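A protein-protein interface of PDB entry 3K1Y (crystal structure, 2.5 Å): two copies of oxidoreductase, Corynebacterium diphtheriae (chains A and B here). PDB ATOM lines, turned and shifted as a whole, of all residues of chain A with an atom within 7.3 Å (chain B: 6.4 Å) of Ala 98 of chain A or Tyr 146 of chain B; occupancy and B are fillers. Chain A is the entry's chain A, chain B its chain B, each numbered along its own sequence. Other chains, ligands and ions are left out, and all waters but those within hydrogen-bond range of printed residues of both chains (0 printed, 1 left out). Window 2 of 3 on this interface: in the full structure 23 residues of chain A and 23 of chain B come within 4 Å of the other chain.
CB of Lys 97 of chain A touches NZ of Lys 105 of chain B, 3.9 Å away.
Leu 143 of chain B touches Lys 97 of chain A.
Tyr 146 of chain B touches Lys 97 of chain A.
SD of Met 147 of chain B touches CE of Lys 97 of chain A (3.8 Å).
Tyr 146 of chain B touches Ala 98 of chain A.
Arg 131 of chain A touches Tyr 146 of chain B (NH2 to OH, 3.5 Å).
His 132 of chain A touches Tyr 146 of chain B (CE1 to CE1, 3.8 Å).
O of Phe 96 of chain A sits at hydrogen-bond distance from NZ of Lys 105 of chain B (2.7 Å).
O of Tyr 100 of chain A sits at hydrogen-bond distance from NZ of Lys 105 of chain B (3.1 Å).
No position is printed for both chains.
Ala 98 of chain A touches just one residue of chain B: Tyr 146.
Of the printed residues of chain B, Arg 131 of chain A touches Tyr 146.
Val 135 of chain A touches none of the printed residues of chain B.
Tyr 146 of chain B touches four residues of chain A.
Printed residues of chain A within 4 Å of Met 147 of chain B: Lys 97 (3.8 Å).
The nearest residue of chain B that does not touch Ala 98 of chain A is Pro 142 of chain B (5.1 Å).
The nearest residue of chain A that does not touch Tyr 146 of chain B is Phe 96 of chain A (5.7 Å).
The nearest printed residue of chain A that does not touch Met 147 of chain B is Ala 98 of chain A (7.2 Å).
Of the 11 printed residues of chain B, 4 touch a printed residue of chain A.
Printed residues of chain B that touch a printed residue of chain A: Lys 105, Leu 143, Tyr 146 and Met 147.
Hydrophobic or aromatic side chains of chain B that line the printed part of chain A: Leu 143, Tyr 146 and Met 147.
Along chain B the printed residues that touch a printed residue of chain A span positions 105 to 147.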
ATOM      1  N   VAL A  95     -25.186  17.026 -24.896  1.00  0.00           N
ATOM      2  CA  VAL A  95     -24.508  18.167 -25.485  1.00  0.00           C
ATOM      3  C   VAL A  95     -23.015  17.942 -25.462  1.00  0.00           C
ATOM      4  O   VAL A  95     -22.415  17.821 -24.398  1.00  0.00           O
ATOM      5  CB  VAL A  95     -24.840  19.464 -24.739  1.00  0.00           C
ATOM      6  CG1 VAL A  95     -24.232  20.658 -25.488  1.00  0.00           C
ATOM      7  CG2 VAL A  95     -26.351  19.610 -24.607  1.00  0.00           C
ATOM      8  N   PHE A  96     -22.424  17.854 -26.649  1.00  0.00           N
ATOM      9  CA  PHE A  96     -20.991  17.641 -26.782  1.00  0.00           C
ATOM     10  C   PHE A  96     -20.434  18.875 -27.468  1.00  0.00           C
ATOM     11  O   PHE A  96     -20.996  19.351 -28.453  1.00  0.00           O
ATOM     12  CB  PHE A  96     -20.693  16.396 -27.637  1.00  0.00           C
ATOM     13  CG  PHE A  96     -21.050  15.087 -26.978  1.00  0.00           C
ATOM     14  CD1 PHE A  96     -21.702  15.049 -25.751  1.00  0.00           C
ATOM     15  CD2 PHE A  96     -20.763  13.882 -27.618  1.00  0.00           C
ATOM     16  CE1 PHE A  96     -22.066  13.836 -25.170  1.00  0.00           C
ATOM     17  CE2 PHE A  96     -21.122  12.663 -27.047  1.00  0.00           C
ATOM     18  CZ  PHE A  96     -21.777  12.642 -25.821  1.00  0.00           C
ATOM     19  N   LYS A  97     -19.327  19.383 -26.940  1.00  0.00           N
ATOM     20  CA  LYS A  97     -18.685  20.577 -27.473  1.00  0.00           C
ATOM     21  C   LYS A  97     -19.671  21.704 -27.766  1.00  0.00           C
ATOM     22  O   LYS A  97     -19.587  22.372 -28.788  1.00  0.00           O
ATOM     23  CB  LYS A  97     -17.867  20.235 -28.721  1.00  0.00           C
ATOM     24  CG  LYS A  97     -16.699  19.266 -28.446  1.00  0.00           C
ATOM     25  CD  LYS A  97     -15.882  19.715 -27.234  1.00  0.00           C
ATOM     26  CE  LYS A  97     -14.529  19.014 -27.140  1.00  0.00           C
ATOM     27  NZ  LYS A  97     -14.636  17.541 -27.014  1.00  0.00           N
ATOM     28  N   ALA A  98     -20.615  21.890 -26.847  1.00  0.00           N
ATOM     29  CA  ALA A  98     -21.610  22.963 -26.904  1.00  0.00           C
ATOM     30  C   ALA A  98     -22.673  22.899 -27.995  1.00  0.00           C
ATOM     31  O   ALA A  98     -23.205  23.927 -28.419  1.00  0.00           O
ATOM     32  CB  ALA A  98     -20.892  24.324 -26.949  1.00  0.00           C
ATOM     33  N   SER A  99     -22.996  21.698 -28.445  1.00  0.00           N
ATOM     34  CA  SER A  99     -24.022  21.546 -29.465  1.00  0.00           C
ATOM     35  C   SER A  99     -24.473  20.096 -29.538  1.00  0.00           C
ATOM     36  O   SER A  99     -24.103  19.283 -28.688  1.00  0.00           O
ATOM     37  CB  SER A  99     -23.491  22.013 -30.822  1.00  0.00           C
ATOM     38  OG  SER A  99     -24.504  21.939 -31.806  1.00  0.00           O
ATOM     39  N   TYR A 100     -25.285  19.765 -30.534  1.00  0.00           N
ATOM     40  CA  TYR A 100     -25.754  18.392 -30.662  1.00  0.00           C
ATOM     41  C   TYR A 100     -24.596  17.477 -31.027  1.00  0.00           C
ATOM     42  O   TYR A 100     -23.575  17.931 -31.542  1.00  0.00           O
ATOM     43  CB  TYR A 100     -26.882  18.292 -31.691  1.00  0.00           C
ATOM     44  CG  TYR A 100     -26.592  18.874 -33.050  1.00  0.00           C
ATOM     45  CD1 TYR A 100     -25.494  18.447 -33.803  1.00  0.00           C
ATOM     46  CD2 TYR A 100     -27.464  19.795 -33.624  1.00  0.00           C
ATOM     47  CE1 TYR A 100     -25.281  18.920 -35.102  1.00  0.00           C
ATOM     48  CE2 TYR A 100     -27.262  20.275 -34.913  1.00  0.00           C
ATOM     49  CZ  TYR A 100     -26.173  19.832 -35.646  1.00  0.00           C
ATOM     50  OH  TYR A 100     -25.998  20.287 -36.932  1.00  0.00           O
ATOM     51  N   ARG A 131     -26.423  26.094 -18.796  1.00  0.00           N
ATOM     52  CA  ARG A 131     -25.693  27.143 -19.505  1.00  0.00           C
ATOM     53  C   ARG A 131     -25.786  27.033 -21.027  1.00  0.00           C
ATOM     54  O   ARG A 131     -25.729  28.039 -21.731  1.00  0.00           O
ATOM     55  CB  ARG A 131     -24.223  27.189 -19.046  1.00  0.00           C
ATOM     56  CG  ARG A 131     -23.357  25.983 -19.389  1.00  0.00           C
ATOM     57  CD  ARG A 131     -22.136  25.964 -18.458  1.00  0.00           C
ATOM     58  NE  ARG A 131     -20.914  25.486 -19.101  1.00  0.00           N
ATOM     59  CZ  ARG A 131     -20.603  24.207 -19.303  1.00  0.00           C
ATOM     60  NH1 ARG A 131     -21.424  23.233 -18.907  1.00  0.00           N
ATOM     61  NH2 ARG A 131     -19.457  23.903 -19.905  1.00  0.00           N
ATOM     62  N   HIS A 132     -25.962  25.813 -21.522  1.00  0.00           N
ATOM     63  CA  HIS A 132     -26.066  25.570 -22.955  1.00  0.00           C
ATOM     64  C   HIS A 132     -27.506  25.313 -23.424  1.00  0.00           C
ATOM     65  O   HIS A 132     -27.727  24.756 -24.502  1.00  0.00           O
ATOM     66  CB  HIS A 132     -25.168  24.383 -23.331  1.00  0.00           C
ATOM     67  CG  HIS A 132     -23.710  24.648 -23.116  1.00  0.00           C
ATOM     68  ND1 HIS A 132     -22.797  23.645 -22.861  1.00  0.00           N
ATOM     69  CD2 HIS A 132     -23.008  25.806 -23.109  1.00  0.00           C
ATOM     70  CE1 HIS A 132     -21.600  24.176 -22.703  1.00  0.00           C
ATOM     71  NE2 HIS A 132     -21.700  25.487 -22.848  1.00  0.00           N
ATOM     72  N   LEU A 134     -29.502  27.084 -24.868  1.00  0.00           N
ATOM     73  CA  LEU A 134     -29.812  27.657 -26.184  1.00  0.00           C
ATOM     74  C   LEU A 134     -29.345  26.763 -27.336  1.00  0.00           C
ATOM     75  O   LEU A 134     -29.383  27.164 -28.503  1.00  0.00           O
ATOM     76  CB  LEU A 134     -29.214  29.068 -26.340  1.00  0.00           C
ATOM     77  CG  LEU A 134     -29.725  30.198 -25.429  1.00  0.00           C
ATOM     78  CD1 LEU A 134     -29.044  31.498 -25.809  1.00  0.00           C
ATOM     79  CD2 LEU A 134     -31.223  30.352 -25.554  1.00  0.00           C
ATOM     80  N   VAL A 135     -28.898  25.555 -27.016  1.00  0.00           N
ATOM     81  CA  VAL A 135     -28.484  24.629 -28.061  1.00  0.00           C
ATOM     82  C   VAL A 135     -29.745  24.228 -28.821  1.00  0.00           C
ATOM     83  O   VAL A 135     -29.683  23.785 -29.961  1.00  0.00           O
ATOM     84  CB  VAL A 135     -27.827  23.355 -27.491  1.00  0.00           C
ATOM     85  CG1 VAL A 135     -28.838  22.569 -26.661  1.00  0.00           C
ATOM     86  CG2 VAL A 135     -27.302  22.505 -28.627  1.00  0.00           C
ATOM     87  N   ALA A 139     -29.222  25.339 -32.699  1.00  0.00           N
ATOM     88  CA  ALA A 139     -28.651  24.165 -33.353  1.00  0.00           C
ATOM     89  C   ALA A 139     -29.712  23.147 -33.786  1.00  0.00           C
ATOM     90  O   ALA A 139     -29.767  22.792 -34.962  1.00  0.00           O
ATOM     91  CB  ALA A 139     -27.614  23.501 -32.444  1.00  0.00           C
ATOM     92  N   LYS B 105     -18.328  16.815 -36.814  1.00  0.00           N
ATOM     93  CA  LYS B 105     -18.564  17.072 -35.401  1.00  0.00           C
ATOM     94  C   LYS B 105     -18.113  15.923 -34.497  1.00  0.00           C
ATOM     95  O   LYS B 105     -17.787  16.141 -33.321  1.00  0.00           O
ATOM     96  CB  LYS B 105     -20.048  17.354 -35.175  1.00  0.00           C
ATOM     97  CG  LYS B 105     -20.426  17.701 -33.742  1.00  0.00           C
ATOM     98  CD  LYS B 105     -19.691  18.937 -33.243  1.00  0.00           C
ATOM     99  CE  LYS B 105     -20.311  19.455 -31.942  1.00  0.00           C
ATOM    100  NZ  LYS B 105     -20.523  18.368 -30.917  1.00  0.00           N
ATOM    101  N   THR B 113     -10.891  17.985 -23.786  1.00  0.00           N
ATOM    102  CA  THR B 113     -11.356  19.330 -23.502  1.00  0.00           C
ATOM    103  C   THR B 113     -10.320  20.402 -23.826  1.00  0.00           C
ATOM    104  O   THR B 113     -10.655  21.430 -24.401  1.00  0.00           O
ATOM    105  CB  THR B 113     -11.733  19.459 -22.029  1.00  0.00           C
ATOM    106  OG1 THR B 113     -12.598  18.378 -21.680  1.00  0.00           O
ATOM    107  CG2 THR B 113     -12.444  20.772 -21.771  1.00  0.00           C
ATOM    108  N   ARG B 141     -17.691  28.443 -35.928  1.00  0.00           N
ATOM    109  CA  ARG B 141     -17.097  29.419 -35.031  1.00  0.00           C
ATOM    110  C   ARG B 141     -17.450  29.101 -33.573  1.00  0.00           C
ATOM    111  O   ARG B 141     -16.579  29.104 -32.696  1.00  0.00           O
ATOM    112  CB  ARG B 141     -17.559  30.829 -35.419  1.00  0.00           C
ATOM    113  CG  ARG B 141     -16.605  31.903 -34.964  1.00  0.00           C
ATOM    114  CD  ARG B 141     -16.499  33.051 -35.964  1.00  0.00           C
ATOM    115  NE  ARG B 141     -15.228  33.716 -35.756  1.00  0.00           N
ATOM    116  CZ  ARG B 141     -14.366  34.030 -36.715  1.00  0.00           C
ATOM    117  NH1 ARG B 141     -14.630  33.758 -37.989  1.00  0.00           N
ATOM    118  NH2 ARG B 141     -13.201  34.571 -36.379  1.00  0.00           N
ATOM    119  N   PRO B 142     -18.736  28.823 -33.295  1.00  0.00           N
ATOM    120  CA  PRO B 142     -19.126  28.505 -31.916  1.00  0.00           C
ATOM    121  C   PRO B 142     -18.455  27.211 -31.473  1.00  0.00           C
ATOM    122  O   PRO B 142     -18.155  27.023 -30.297  1.00  0.00           O
ATOM    123  CB  PRO B 142     -20.644  28.377 -32.006  1.00  0.00           C
ATOM    124  CG  PRO B 142     -20.984  29.367 -33.105  1.00  0.00           C
ATOM    125  CD  PRO B 142     -19.925  29.048 -34.137  1.00  0.00           C
ATOM    126  N   LEU B 143     -18.206  26.324 -32.427  1.00  0.00           N
ATOM    127  CA  LEU B 143     -17.548  25.060 -32.115  1.00  0.00           C
ATOM    128  C   LEU B 143     -16.104  25.306 -31.691  1.00  0.00           C
ATOM    129  O   LEU B 143     -15.735  25.040 -30.547  1.00  0.00           O
ATOM    130  CB  LEU B 143     -17.584  24.127 -33.322  1.00  0.00           C
ATOM    131  CG  LEU B 143     -16.870  22.801 -33.096  1.00  0.00           C
ATOM    132  CD1 LEU B 143     -17.327  22.183 -31.799  1.00  0.00           C
ATOM    133  CD2 LEU B 143     -17.137  21.879 -34.270  1.00  0.00           C
ATOM    134  N   LEU B 144     -15.295  25.829 -32.609  1.00  0.00           N
ATOM    135  CA  LEU B 144     -13.893  26.113 -32.321  1.00  0.00           C
ATOM    136  C   LEU B 144     -13.708  27.107 -31.169  1.00  0.00           C
ATOM    137  O   LEU B 144     -12.670  27.102 -30.500  1.00  0.00           O
ATOM    138  CB  LEU B 144     -13.191  26.634 -33.579  1.00  0.00           C
ATOM    139  CG  LEU B 144     -12.717  25.595 -34.595  1.00  0.00           C
ATOM    140  CD1 LEU B 144     -11.512  24.867 -34.031  1.00  0.00           C
ATOM    141  CD2 LEU B 144     -13.846  24.614 -34.929  1.00  0.00           C
ATOM    142  N   SER B 145     -14.703  27.958 -30.938  1.00  0.00           N
ATOM    143  CA  SER B 145     -14.612  28.920 -29.842  1.00  0.00           C
ATOM    144  C   SER B 145     -14.777  28.194 -28.529  1.00  0.00           C
ATOM    145  O   SER B 145     -14.097  28.497 -27.556  1.00  0.00           O
ATOM    146  CB  SER B 145     -15.691  29.997 -29.949  1.00  0.00           C
ATOM    147  OG  SER B 145     -15.168  31.155 -30.567  1.00  0.00           O
ATOM    148  N   TYR B 146     -15.695  27.237 -28.496  1.00  0.00           N
ATOM    149  CA  TYR B 146     -15.905  26.472 -27.277  1.00  0.00           C
ATOM    150  C   TYR B 146     -14.587  25.841 -26.835  1.00  0.00           C
ATOM    151  O   TYR B 146     -14.290  25.766 -25.640  1.00  0.00           O
ATOM    152  CB  TYR B 146     -16.925  25.358 -27.495  1.00  0.00           C
ATOM    153  CG  TYR B 146     -17.179  24.578 -26.240  1.00  0.00           C
ATOM    154  CD1 TYR B 146     -17.856  25.161 -25.164  1.00  0.00           C
ATOM    155  CD2 TYR B 146     -16.712  23.276 -26.101  1.00  0.00           C
ATOM    156  CE1 TYR B 146     -18.057  24.467 -23.977  1.00  0.00           C
ATOM    157  CE2 TYR B 146     -16.910  22.570 -24.918  1.00  0.00           C
ATOM    158  CZ  TYR B 146     -17.582  23.176 -23.861  1.00  0.00           C
ATOM    159  OH  TYR B 146     -17.775  22.488 -22.687  1.00  0.00           O
ATOM    160  N   MET B 147     -13.801  25.391 -27.808  1.00  0.00           N
ATOM    161  CA  MET B 147     -12.528  24.757 -27.519  1.00  0.00           C
ATOM    162  C   MET B 147     -11.397  25.761 -27.327  1.00  0.00           C
ATOM    163  O   MET B 147     -10.214  25.419 -27.350  1.00  0.00           O
ATOM    164  CB  MET B 147     -12.209  23.745 -28.620  1.00  0.00           C
ATOM    165  CG  MET B 147     -13.203  22.594 -28.620  1.00  0.00           C
ATOM    166  SD  MET B 147     -12.774  21.108 -29.768  1.00  0.00           S
ATOM    167  CE  MET B 147     -14.148  21.363 -31.091  1.00  0.00           C
ATOM    168  N   ARG B 148     -11.788  27.012 -27.133  1.00  0.00           N
ATOM    169  CA  ARG B 148     -10.856  28.105 -26.890  1.00  0.00           C
ATOM    170  C   ARG B 148      -9.810  28.352 -27.971  1.00  0.00           C
ATOM    171  O   ARG B 148      -8.732  28.899 -27.696  1.00  0.00           O
ATOM    172  CB  ARG B 148     -10.178  27.889 -25.541  1.00  0.00           C
ATOM    173  CG  ARG B 148     -11.168  27.876 -24.407  1.00  0.00           C
ATOM    174  CD  ARG B 148     -10.510  27.593 -23.081  1.00  0.00           C
ATOM    175  NE  ARG B 148      -9.310  28.389 -22.843  1.00  0.00           N
ATOM    176  CZ  ARG B 148      -8.683  28.431 -21.674  1.00  0.00           C
ATOM    177  NH1 ARG B 148      -9.155  27.731 -20.652  1.00  0.00           N
ATOM    178  NH2 ARG B 148      -7.582  29.153 -21.529  1.00  0.00           N
ATOM    179  N   ALA B 149     -10.124  27.955 -29.198  1.00  0.00           N
ATOM    180  CA  ALA B 149      -9.203  28.177 -30.296  1.00  0.00           C
ATOM    181  C   ALA B 149      -9.439  29.602 -30.783  1.00  0.00           C
ATOM    182  O   ALA B 149     -10.565  30.078 -30.775  1.00  0.00           O
ATOM    183  CB  ALA B 149      -9.476  27.186 -31.416  1.00  0.00           C
